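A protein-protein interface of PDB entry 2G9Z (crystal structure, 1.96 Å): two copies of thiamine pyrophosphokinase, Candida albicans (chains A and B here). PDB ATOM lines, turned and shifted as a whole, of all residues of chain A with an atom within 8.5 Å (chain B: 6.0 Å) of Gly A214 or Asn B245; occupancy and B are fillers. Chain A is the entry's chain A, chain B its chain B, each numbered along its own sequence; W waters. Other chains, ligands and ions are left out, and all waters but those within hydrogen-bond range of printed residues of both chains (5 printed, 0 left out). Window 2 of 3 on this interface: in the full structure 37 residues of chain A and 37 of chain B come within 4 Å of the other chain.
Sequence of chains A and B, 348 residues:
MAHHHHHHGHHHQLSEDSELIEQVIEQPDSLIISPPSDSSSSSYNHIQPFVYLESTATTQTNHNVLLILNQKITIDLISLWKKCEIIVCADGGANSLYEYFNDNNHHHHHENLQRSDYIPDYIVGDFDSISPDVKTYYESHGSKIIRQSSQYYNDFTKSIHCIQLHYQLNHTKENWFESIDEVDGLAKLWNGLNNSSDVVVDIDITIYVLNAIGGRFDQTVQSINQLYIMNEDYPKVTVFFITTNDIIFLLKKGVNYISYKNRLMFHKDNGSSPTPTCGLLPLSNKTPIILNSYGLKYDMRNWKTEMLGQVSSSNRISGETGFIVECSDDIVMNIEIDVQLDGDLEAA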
ATOM      1  N   ASN A  70      -5.697   4.175   6.749  1.00  0.00           N
ATOM      2  CA  ASN A  70      -6.500   5.108   7.525  1.00  0.00           C
ATOM      3  C   ASN A  70      -5.848   6.242   8.325  1.00  0.00           C
ATOM      4  O   ASN A  70      -5.610   6.115   9.524  1.00  0.00           O
ATOM      5  CB  ASN A  70      -7.416   4.293   8.441  1.00  0.00           C
ATOM      6  CG  ASN A  70      -8.499   5.136   9.085  1.00  0.00           C
ATOM      7  OD1 ASN A  70      -8.879   6.185   8.564  1.00  0.00           O
ATOM      8  ND2 ASN A  70      -9.014   4.670  10.216  1.00  0.00           N
ATOM      9  N   GLN A  71      -5.596   7.359   7.645  1.00  0.00           N
ATOM     10  CA  GLN A  71      -5.030   8.563   8.250  1.00  0.00           C
ATOM     11  C   GLN A  71      -5.284   9.729   7.301  1.00  0.00           C
ATOM     12  O   GLN A  71      -5.393   9.543   6.090  1.00  0.00           O
ATOM     13  CB  GLN A  71      -3.521   8.415   8.523  1.00  0.00           C
ATOM     14  CG  GLN A  71      -3.197   7.717   9.847  1.00  0.00           C
ATOM     15  CD  GLN A  71      -1.719   7.781  10.215  1.00  0.00           C
ATOM     16  OE1 GLN A  71      -0.902   7.015   9.702  1.00  0.00           O
ATOM     17  NE2 GLN A  71      -1.372   8.707  11.103  1.00  0.00           N
ATOM     18  N   ASN A 211      -0.307   6.651   4.722  1.00  0.00           N
ATOM     19  CA  ASN A 211      -0.870   6.473   6.064  1.00  0.00           C
ATOM     20  C   ASN A 211      -0.565   5.177   6.818  1.00  0.00           C
ATOM     21  O   ASN A 211      -1.292   4.818   7.752  1.00  0.00           O
ATOM     22  CB  ASN A 211      -2.393   6.661   5.999  1.00  0.00           C
ATOM     23  CG  ASN A 211      -2.793   7.935   5.270  1.00  0.00           C
ATOM     24  OD1 ASN A 211      -2.188   8.991   5.467  1.00  0.00           O
ATOM     25  ND2 ASN A 211      -3.823   7.842   4.425  1.00  0.00           N
ATOM     26  N   ALA A 212       0.500   4.482   6.438  1.00  0.00           N
ATOM     27  CA  ALA A 212       0.865   3.230   7.102  1.00  0.00           C
ATOM     28  C   ALA A 212       1.883   3.466   8.213  1.00  0.00           C
ATOM     29  O   ALA A 212       2.138   2.587   9.040  1.00  0.00           O
ATOM     30  CB  ALA A 212       1.434   2.249   6.085  1.00  0.00           C
ATOM     31  N   ILE A 213       2.462   4.660   8.218  1.00  0.00           N
ATOM     32  CA  ILE A 213       3.462   5.041   9.205  1.00  0.00           C
ATOM     33  C   ILE A 213       2.974   6.268   9.966  1.00  0.00           C
ATOM     34  O   ILE A 213       2.207   7.068   9.432  1.00  0.00           O
ATOM     35  CB  ILE A 213       4.806   5.406   8.512  1.00  0.00           C
ATOM     36  CG1 ILE A 213       5.271   4.251   7.621  1.00  0.00           C
ATOM     37  CG2 ILE A 213       5.859   5.757   9.557  1.00  0.00           C
ATOM     38  CD1 ILE A 213       5.594   2.966   8.371  1.00  0.00           C
ATOM     39  N   GLY A 214       3.405   6.405  11.217  1.00  0.00           N
ATOM     40  CA  GLY A 214       3.031   7.568  12.002  1.00  0.00           C
ATOM     41  C   GLY A 214       1.780   7.498  12.854  1.00  0.00           C
ATOM     42  O   GLY A 214       1.547   8.386  13.673  1.00  0.00           O
ATOM     43  N   GLY A 215       0.966   6.464  12.667  1.00  0.00           N
ATOM     44  CA  GLY A 215      -0.246   6.341  13.459  1.00  0.00           C
ATOM     45  C   GLY A 215       0.013   5.445  14.653  1.00  0.00           C
ATOM     46  O   GLY A 215       1.038   5.577  15.321  1.00  0.00           O
ATOM     47  N   ARG A 216      -0.908   4.527  14.925  1.00  0.00           N
ATOM     48  CA  ARG A 216      -0.741   3.603  16.038  1.00  0.00           C
ATOM     49  C   ARG A 216       0.590   2.882  15.788  1.00  0.00           C
ATOM     50  O   ARG A 216       0.830   2.351  14.700  1.00  0.00           O
ATOM     51  CB  ARG A 216      -1.905   2.618  16.067  1.00  0.00           C
ATOM     52  CG  ARG A 216      -2.297   2.145  17.453  1.00  0.00           C
ATOM     53  CD  ARG A 216      -3.504   1.234  17.352  1.00  0.00           C
ATOM     54  NE  ARG A 216      -3.167  -0.003  16.653  1.00  0.00           N
ATOM     55  CZ  ARG A 216      -4.034  -0.726  15.956  1.00  0.00           C
ATOM     56  NH1 ARG A 216      -5.300  -0.336  15.852  1.00  0.00           N
ATOM     57  NH2 ARG A 216      -3.640  -1.850  15.381  1.00  0.00           N
ATOM     58  N   PHE A 217       1.455   2.874  16.795  1.00  0.00           N
ATOM     59  CA  PHE A 217       2.778   2.277  16.663  1.00  0.00           C
ATOM     60  C   PHE A 217       2.861   0.814  16.229  1.00  0.00           C
ATOM     61  O   PHE A 217       3.753   0.452  15.455  1.00  0.00           O
ATOM     62  CB  PHE A 217       3.567   2.467  17.957  1.00  0.00           C
ATOM     63  CG  PHE A 217       5.041   2.332  17.776  1.00  0.00           C
ATOM     64  CD1 PHE A 217       5.717   3.166  16.890  1.00  0.00           C
ATOM     65  CD2 PHE A 217       5.758   1.366  18.468  1.00  0.00           C
ATOM     66  CE1 PHE A 217       7.094   3.036  16.696  1.00  0.00           C
ATOM     67  CE2 PHE A 217       7.135   1.230  18.279  1.00  0.00           C
ATOM     68  CZ  PHE A 217       7.799   2.067  17.392  1.00  0.00           C
ATOM     69  N   ASP A 218       1.955  -0.034  16.707  1.00  0.00           N
ATOM     70  CA  ASP A 218       2.015  -1.439  16.307  1.00  0.00           C
ATOM     71  C   ASP A 218       1.742  -1.583  14.809  1.00  0.00           C
ATOM     72  O   ASP A 218       2.231  -2.517  14.171  1.00  0.00           O
ATOM     73  CB  ASP A 218       1.038  -2.296  17.127  1.00  0.00           C
ATOM     74  CG  ASP A 218      -0.417  -1.894  16.932  1.00  0.00           C
ATOM     75  OD1 ASP A 218      -0.759  -0.725  17.182  1.00  0.00           O
ATOM     76  OD2 ASP A 218      -1.222  -2.759  16.534  1.00  0.00           O
ATOM     77  N   GLN A 219       0.970  -0.649  14.257  1.00  0.00           N
ATOM     78  CA  GLN A 219       0.652  -0.641  12.833  1.00  0.00           C
ATOM     79  C   GLN A 219       1.914  -0.251  12.063  1.00  0.00           C
ATOM     80  O   GLN A 219       2.220  -0.807  11.013  1.00  0.00           O
ATOM     81  CB  GLN A 219      -0.458   0.373  12.549  1.00  0.00           C
ATOM     82  CG  GLN A 219      -0.608   0.741  11.077  1.00  0.00           C
ATOM     83  CD  GLN A 219      -1.498   1.951  10.859  1.00  0.00           C
ATOM     84  OE1 GLN A 219      -1.688   2.399   9.728  1.00  0.00           O
ATOM     85  NE2 GLN A 219      -2.047   2.488  11.944  1.00  0.00           N
ATOM     86  N   THR A 220       2.636   0.727  12.596  1.00  0.00           N
ATOM     87  CA  THR A 220       3.867   1.183  11.978  1.00  0.00           C
ATOM     88  C   THR A 220       4.855   0.026  11.933  1.00  0.00           C
ATOM     89  O   THR A 220       5.451  -0.250  10.895  1.00  0.00           O
ATOM     90  CB  THR A 220       4.484   2.344  12.778  1.00  0.00           C
ATOM     91  OG1 THR A 220       3.641   3.493  12.653  1.00  0.00           O
ATOM     92  CG2 THR A 220       5.888   2.673  12.267  1.00  0.00           C
ATOM     93  N   VAL A 221       5.010  -0.659  13.059  1.00  0.00           N
ATOM     94  CA  VAL A 221       5.937  -1.771  13.125  1.00  0.00           C
ATOM     95  C   VAL A 221       5.514  -2.916  12.212  1.00  0.00           C
ATOM     96  O   VAL A 221       6.350  -3.495  11.515  1.00  0.00           O
ATOM     97  CB  VAL A 221       6.102  -2.263  14.583  1.00  0.00           C
ATOM     98  CG1 VAL A 221       6.944  -3.536  14.620  1.00  0.00           C
ATOM     99  CG2 VAL A 221       6.776  -1.170  15.405  1.00  0.00           C
ATOM    100  N   SER A 223       3.865  -2.712   9.496  1.00  0.00           N
ATOM    101  CA  SER A 223       4.119  -2.298   8.116  1.00  0.00           C
ATOM    102  C   SER A 223       5.580  -2.528   7.748  1.00  0.00           C
ATOM    103  O   SER A 223       5.891  -3.025   6.669  1.00  0.00           O
ATOM    104  CB  SER A 223       3.763  -0.821   7.924  1.00  0.00           C
ATOM    105  OG  SER A 223       2.373  -0.605   8.095  1.00  0.00           O
ATOM    106  N   PHE A 241       6.813   3.768   1.283  1.00  0.00           N
ATOM    107  CA  PHE A 241       5.875   4.316   2.246  1.00  0.00           C
ATOM    108  C   PHE A 241       6.060   5.819   2.147  1.00  0.00           C
ATOM    109  O   PHE A 241       7.166   6.332   2.360  1.00  0.00           O
ATOM    110  CB  PHE A 241       6.210   3.873   3.675  1.00  0.00           C
ATOM    111  CG  PHE A 241       5.893   2.443   3.962  1.00  0.00           C
ATOM    112  CD1 PHE A 241       4.575   2.017   4.084  1.00  0.00           C
ATOM    113  CD2 PHE A 241       6.914   1.520   4.135  1.00  0.00           C
ATOM    114  CE1 PHE A 241       4.281   0.683   4.375  1.00  0.00           C
ATOM    115  CE2 PHE A 241       6.631   0.186   4.427  1.00  0.00           C
ATOM    116  CZ  PHE A 241       5.316  -0.231   4.546  1.00  0.00           C
ATOM    117  N   ILE A 242       4.999   6.531   1.791  1.00  0.00           N
ATOM    118  CA  ILE A 242       5.087   7.978   1.699  1.00  0.00           C
ATOM    119  C   ILE A 242       4.308   8.521   2.880  1.00  0.00           C
ATOM    120  O   ILE A 242       3.117   8.245   3.024  1.00  0.00           O
ATOM    121  CB  ILE A 242       4.481   8.510   0.386  1.00  0.00           C
ATOM    122  CG1 ILE A 242       5.340   8.066  -0.802  1.00  0.00           C
ATOM    123  CG2 ILE A 242       4.395  10.036   0.435  1.00  0.00           C
ATOM    124  CD1 ILE A 242       4.778   8.481  -2.148  1.00  0.00           C
ATOM    125  N   THR A 243       4.988   9.267   3.742  1.00  0.00           N
ATOM    126  CA  THR A 243       4.338   9.825   4.919  1.00  0.00           C
ATOM    127  C   THR A 243       4.327  11.335   4.848  1.00  0.00           C
ATOM    128  O   THR A 243       4.739  11.926   3.852  1.00  0.00           O
ATOM    129  CB  THR A 243       5.062   9.416   6.217  1.00  0.00           C
ATOM    130  OG1 THR A 243       6.240  10.218   6.383  1.00  0.00           O
ATOM    131  CG2 THR A 243       5.463   7.949   6.156  1.00  0.00           C
ATOM    132  N   THR A 244       3.855  11.953   5.922  1.00  0.00           N
ATOM    133  CA  THR A 244       3.787  13.402   6.002  1.00  0.00           C
ATOM    134  C   THR A 244       5.194  13.988   6.098  1.00  0.00           C
ATOM    135  O   THR A 244       5.457  15.095   5.631  1.00  0.00           O
ATOM    136  CB  THR A 244       2.985  13.838   7.241  1.00  0.00           C
ATOM    137  OG1 THR A 244       1.639  13.364   7.127  1.00  0.00           O
ATOM    138  CG2 THR A 244       2.975  15.356   7.368  1.00  0.00           C
ATOM    139  N   ASN A 245       6.103  13.219   6.680  1.00  0.00           N
ATOM    140  CA  ASN A 245       7.468  13.680   6.875  1.00  0.00           C
ATOM    141  C   ASN A 245       8.516  13.126   5.923  1.00  0.00           C
ATOM    142  O   ASN A 245       9.508  13.799   5.628  1.00  0.00           O
ATOM    143  CB  ASN A 245       7.884  13.362   8.309  1.00  0.00           C
ATOM    144  CG  ASN A 245       6.905  13.908   9.321  1.00  0.00           C
ATOM    145  OD1 ASN A 245       6.856  15.114   9.555  1.00  0.00           O
ATOM    146  ND2 ASN A 245       6.099  13.025   9.908  1.00  0.00           N
ATOM    147  N   ASP A 246       8.297  11.915   5.429  1.00  0.00           N
ATOM    148  CA  ASP A 246       9.293  11.296   4.575  1.00  0.00           C
ATOM    149  C   ASP A 246       8.804  10.172   3.670  1.00  0.00           C
ATOM    150  O   ASP A 246       7.612   9.894   3.568  1.00  0.00           O
ATOM    151  CB  ASP A 246      10.401  10.744   5.477  1.00  0.00           C
ATOM    152  CG  ASP A 246       9.845   9.961   6.667  1.00  0.00           C
ATOM    153  OD1 ASP A 246       8.930   9.136   6.460  1.00  0.00           O
ATOM    154  OD2 ASP A 246      10.318  10.160   7.809  1.00  0.00           O
ATOM    155  N   ILE A 248       9.850   6.129   2.876  1.00  0.00           N
ATOM    156  CA  ILE A 248      10.553   5.015   3.492  1.00  0.00           C
ATOM    157  C   ILE A 248      10.585   3.837   2.535  1.00  0.00           C
ATOM    158  O   ILE A 248       9.568   3.476   1.940  1.00  0.00           O
ATOM    159  CB  ILE A 248       9.837   4.623   4.801  1.00  0.00           C
ATOM    160  CG1 ILE A 248       9.716   5.868   5.685  1.00  0.00           C
ATOM    161  CG2 ILE A 248      10.586   3.501   5.513  1.00  0.00           C
ATOM    162  CD1 ILE A 248       8.858   5.680   6.919  1.00  0.00           C
ATOM    163  N   ILE B 213       7.748  10.047  18.944  1.00  0.00           N
ATOM    164  CA  ILE B 213       7.248   9.035  18.021  1.00  0.00           C
ATOM    165  C   ILE B 213       6.267   9.675  17.049  1.00  0.00           C
ATOM    166  O   ILE B 213       5.619  10.663  17.383  1.00  0.00           O
ATOM    167  CB  ILE B 213       6.497   7.916  18.795  1.00  0.00           C
ATOM    168  CG1 ILE B 213       7.411   7.304  19.861  1.00  0.00           C
ATOM    169  CG2 ILE B 213       5.961   6.876  17.825  1.00  0.00           C
ATOM    170  CD1 ILE B 213       8.660   6.618  19.320  1.00  0.00           C
ATOM    171  N   GLY B 214       6.168   9.123  15.844  1.00  0.00           N
ATOM    172  CA  GLY B 214       5.219   9.647  14.878  1.00  0.00           C
ATOM    173  C   GLY B 214       5.702  10.695  13.897  1.00  0.00           C
ATOM    174  O   GLY B 214       5.014  10.985  12.920  1.00  0.00           O
ATOM    175  N   GLY B 215       6.866  11.282  14.153  1.00  0.00           N
ATOM    176  CA  GLY B 215       7.389  12.287  13.246  1.00  0.00           C
ATOM    177  C   GLY B 215       8.330  11.639  12.254  1.00  0.00           C
ATOM    178  O   GLY B 215       8.027  10.576  11.715  1.00  0.00           O
ATOM    179  N   THR B 243       2.209   9.369  23.006  1.00  0.00           N
ATOM    180  CA  THR B 243       1.976   9.964  21.702  1.00  0.00           C
ATOM    181  C   THR B 243       0.516  10.338  21.537  1.00  0.00           C
ATOM    182  O   THR B 243      -0.265  10.277  22.485  1.00  0.00           O
ATOM    183  CB  THR B 243       2.354   8.985  20.573  1.00  0.00           C
ATOM    184  OG1 THR B 243       1.314   8.009  20.419  1.00  0.00           O
ATOM    185  CG2 THR B 243       3.660   8.264  20.914  1.00  0.00           C
ATOM    186  N   THR B 244       0.157  10.721  20.318  1.00  0.00           N
ATOM    187  CA  THR B 244      -1.210  11.103  20.002  1.00  0.00           C
ATOM    188  C   THR B 244      -2.134   9.890  20.011  1.00  0.00           C
ATOM    189  O   THR B 244      -3.317   9.996  20.340  1.00  0.00           O
ATOM    190  CB  THR B 244      -1.291  11.745  18.608  1.00  0.00           C
ATOM    191  OG1 THR B 244      -0.498  12.934  18.581  1.00  0.00           O
ATOM    192  CG2 THR B 244      -2.735  12.094  18.263  1.00  0.00           C
ATOM    193  N   ASN B 245      -1.580   8.733  19.670  1.00  0.00           N
ATOM    194  CA  ASN B 245      -2.366   7.510  19.588  1.00  0.00           C
ATOM    195  C   ASN B 245      -2.176   6.482  20.694  1.00  0.00           C
ATOM    196  O   ASN B 245      -3.071   5.678  20.945  1.00  0.00           O
ATOM    197  CB  ASN B 245      -2.089   6.852  18.239  1.00  0.00           C
ATOM    198  CG  ASN B 245      -2.275   7.812  17.089  1.00  0.00           C
ATOM    199  OD1 ASN B 245      -3.398   8.196  16.768  1.00  0.00           O
ATOM    200  ND2 ASN B 245      -1.172   8.227  16.473  1.00  0.00           N
ATOM    201  N   ASP B 246      -1.028   6.500  21.362  1.00  0.00           N
ATOM    202  CA  ASP B 246      -0.783   5.503  22.394  1.00  0.00           C
ATOM    203  C   ASP B 246       0.337   5.823  23.379  1.00  0.00           C
ATOM    204  O   ASP B 246       0.900   6.915  23.379  1.00  0.00           O
ATOM    205  CB  ASP B 246      -0.466   4.168  21.711  1.00  0.00           C
ATOM    206  CG  ASP B 246       0.561   4.315  20.600  1.00  0.00           C
ATOM    207  OD1 ASP B 246       1.466   5.166  20.741  1.00  0.00           O
ATOM    208  OD2 ASP B 246       0.472   3.581  19.590  1.00  0.00           O
ATOM    209  N   ILE B 247       0.621   4.852  24.243  1.00  0.00           N
ATOM    210  CA  ILE B 247       1.705   4.947  25.205  1.00  0.00           C
ATOM    211  C   ILE B 247       2.589   3.751  24.870  1.00  0.00           C
ATOM    212  O   ILE B 247       2.102   2.634  24.644  1.00  0.00           O
ATOM    213  CB  ILE B 247       1.224   4.874  26.679  1.00  0.00           C
ATOM    214  CG1 ILE B 247       2.433   4.999  27.612  1.00  0.00           C
ATOM    215  CG2 ILE B 247       0.475   3.576  26.941  1.00  0.00           C
ATOM    216  CD1 ILE B 247       2.085   5.431  29.017  1.00  0.00           C
ATOM    217  N   ILE B 335       0.222   0.577  23.832  1.00  0.00           N
ATOM    218  CA  ILE B 335      -1.174   0.423  24.201  1.00  0.00           C
ATOM    219  C   ILE B 335      -1.872   1.675  23.703  1.00  0.00           C
ATOM    220  O   ILE B 335      -1.447   2.786  24.007  1.00  0.00           O
ATOM    221  CB  ILE B 335      -1.364   0.311  25.732  1.00  0.00           C
ATOM    222  CG1 ILE B 335      -0.731  -0.987  26.248  1.00  0.00           C
ATOM    223  CG2 ILE B 335      -2.857   0.326  26.070  1.00  0.00           C
ATOM    224  CD1 ILE B 335      -0.842  -1.177  27.764  1.00  0.00           C
ATOM    225  N   GLU B 336      -2.927   1.498  22.919  1.00  0.00           N
ATOM    226  CA  GLU B 336      -3.651   2.640  22.391  1.00  0.00           C
ATOM    227  C   GLU B 336      -4.375   3.389  23.503  1.00  0.00           C
ATOM    228  O   GLU B 336      -4.887   2.786  24.444  1.00  0.00           O
ATOM    229  CB  GLU B 336      -4.656   2.186  21.323  1.00  0.00           C
ATOM    230  CG  GLU B 336      -5.426   3.331  20.673  1.00  0.00           C
ATOM    231  CD  GLU B 336      -6.167   2.901  19.418  1.00  0.00           C
ATOM    232  OE1 GLU B 336      -6.986   1.960  19.502  1.00  0.00           O
ATOM    233  OE2 GLU B 336      -5.928   3.504  18.349  1.00  0.00           O
ATOM    234  N   ILE B 337      -4.393   4.711  23.397  1.00  0.00           N
ATOM    235  CA  ILE B 337      -5.061   5.557  24.379  1.00  0.00           C
ATOM    236  C   ILE B 337      -6.074   6.411  23.630  1.00  0.00           C
ATOM    237  O   ILE B 337      -5.776   6.938  22.560  1.00  0.00           O
ATOM    238  CB  ILE B 337      -4.062   6.493  25.107  1.00  0.00           C
ATOM    239  CG1 ILE B 337      -3.059   5.660  25.909  1.00  0.00           C
ATOM    240  CG2 ILE B 337      -4.818   7.444  26.031  1.00  0.00           C
ATOM    241  CD1 ILE B 337      -2.006   6.484  26.622  1.00  0.00           C
ATOM    242  N   ASP B 338      -7.269   6.540  24.193  1.00  0.00           N
ATOM    243  CA  ASP B 338      -8.331   7.322  23.572  1.00  0.00           C
ATOM    244  C   ASP B 338      -9.520   7.469  24.512  1.00  0.00           C
ATOM    245  O   ASP B 338      -9.316   7.419  25.742  1.00  0.00           O
ATOM    246  CB  ASP B 338      -8.793   6.658  22.273  1.00  0.00           C
ATOM    247  CG  ASP B 338      -9.335   5.256  22.493  1.00  0.00           C
ATOM    248  OD1 ASP B 338     -10.206   5.080  23.374  1.00  0.00           O
ATOM    249  OD2 ASP B 338      -8.895   4.328  21.780  1.00  0.00           O
HETATM  250  O   HOH W   1       5.112  10.150   9.939  1.00  0.00           O
HETATM  251  O   HOH W   2       7.669   9.060   8.794  1.00  0.00           O
HETATM  252  O   HOH W   3       2.301   6.056  18.284  1.00  0.00           O
HETATM  253  O   HOH W   4       2.040   8.450  16.703  1.00  0.00           O
HETATM  254  O   HOH W   5      -6.529   2.406  16.088  1.00  0.00           O
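The backbone NH (N) of Phe A217 sits at hydrogen-bond distance from the side-chain carboxylate (OD2) of Asp B246, 3.0 Å away.
Gly A214 touches Asn B245 (O to ND2, 3.9 Å). Gly A215 touches Asn B245 (C to ND2, 3.5 Å). Asp B246 touches Arg A216 (OD2 to CA, 3.8 Å). Glu B336 touches Arg A216. Ile B213 touches Phe A217. Asn A245 touches Gly B214. Asn A245 touches Gly B215.
Of the printed residues of chain B, Gly A214 touches Asn B245. Of the printed residues of chain B, Arg A216 touches Asp B246 (3.8 Å) and Glu B336 (3.5 Å). Of the printed residues of chain B, Phe A217 touches Ile B213 (3.8 Å) and Asp B246 (3.0 Å). Of the printed residues of chain B, Asn A245 touches Gly B214 and Gly B215. Ile A248 touches none of the printed residues of chain B. Printed residues of chain A within 4 Å of Ile B213: Phe A217 (3.8 Å). Of the printed residues of chain A, Gly B215 touches Asn A245 (3.5 Å). Thr B243 touches none of the printed residues of chain A. Printed residues of chain A within 4 Å of Asn B245: Gly A214 (3.9 Å) and Gly A215 (3.5 Å). The nearest printed residue of chain A that does not touch Asn B245 is Arg A216 (4.02 Å).
The backbone NH of Gly A214 lies within hydrogen-bond range of the side-chain hydroxyl of Thr A220 (3.3 Å). The guanidinium group (NE) of Arg A216 lies within salt-bridge range of the side-chain carboxylate (OD1) of Asp A218. N of Asn A245 is in hydrogen-bond range of OG1 of Thr A243, 3.0 Å away. The side-chain hydroxyl (OG1) of Thr B243 is in hydrogen-bond range of the backbone NH (N) of Asn B245. The side-chain carboxylate of Asp B246 lies within hydrogen-bond range of the side-chain hydroxyl of Thr B243 (2.9 Å). O of Asn B245 is in hydrogen-bond range of N of Ile B337, at 2.9 Å.
Hydrophobic or aromatic side chains of chain B that line the printed part of chain A: Ile B213. Hydrophobic or aromatic side chains of chain A that line the printed part of chain B: Phe A217. Among the printed residues, no Asp or Glu carboxylate lies within 4 Å of a Lys or Arg side-chain nitrogen of the other chain.
Water W5 bridges the side-chain carboxylate (OE2) of Glu B336 (2.6 Å) and the guanidinium group (NH1) of Arg A216 (3.0 Å). Water W2 lies within hydrogen-bond range of OD1 of Asp A246 (2.7 Å), OG1 of Thr A243 (3.0 Å) and O of Gly B215 (3.3 Å). Water W3 lies within hydrogen-bond range of the side-chain carboxylate (OD1) of Asp B246 (2.7 Å), the side-chain hydroxyl (OG1) of Thr B243 (3.1 Å) and the backbone carbonyl oxygen (O) of Gly A215 (3.3 Å). Water W1 lies within hydrogen-bond range of the side-chain amide nitrogen of Asn A245, the backbone carbonyl oxygen of Gly B214 and the backbone carbonyl oxygen of Gly B215. Water W4 lies within hydrogen-bond range of O of Gly A214 (3.1 Å), ND2 of Asn B245 (3.2 Å) and O of Gly A215 (3.3 Å).
Gly A214 touches Asn B245, and with the chains exchanged Asn A245 touches Gly B214. Gly A215 touches Asn B245, and with the chains exchanged Asn A245 touches Gly B215. Positions printed for both chains: 213, 214, 215, 243, 244, 245 and 246.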
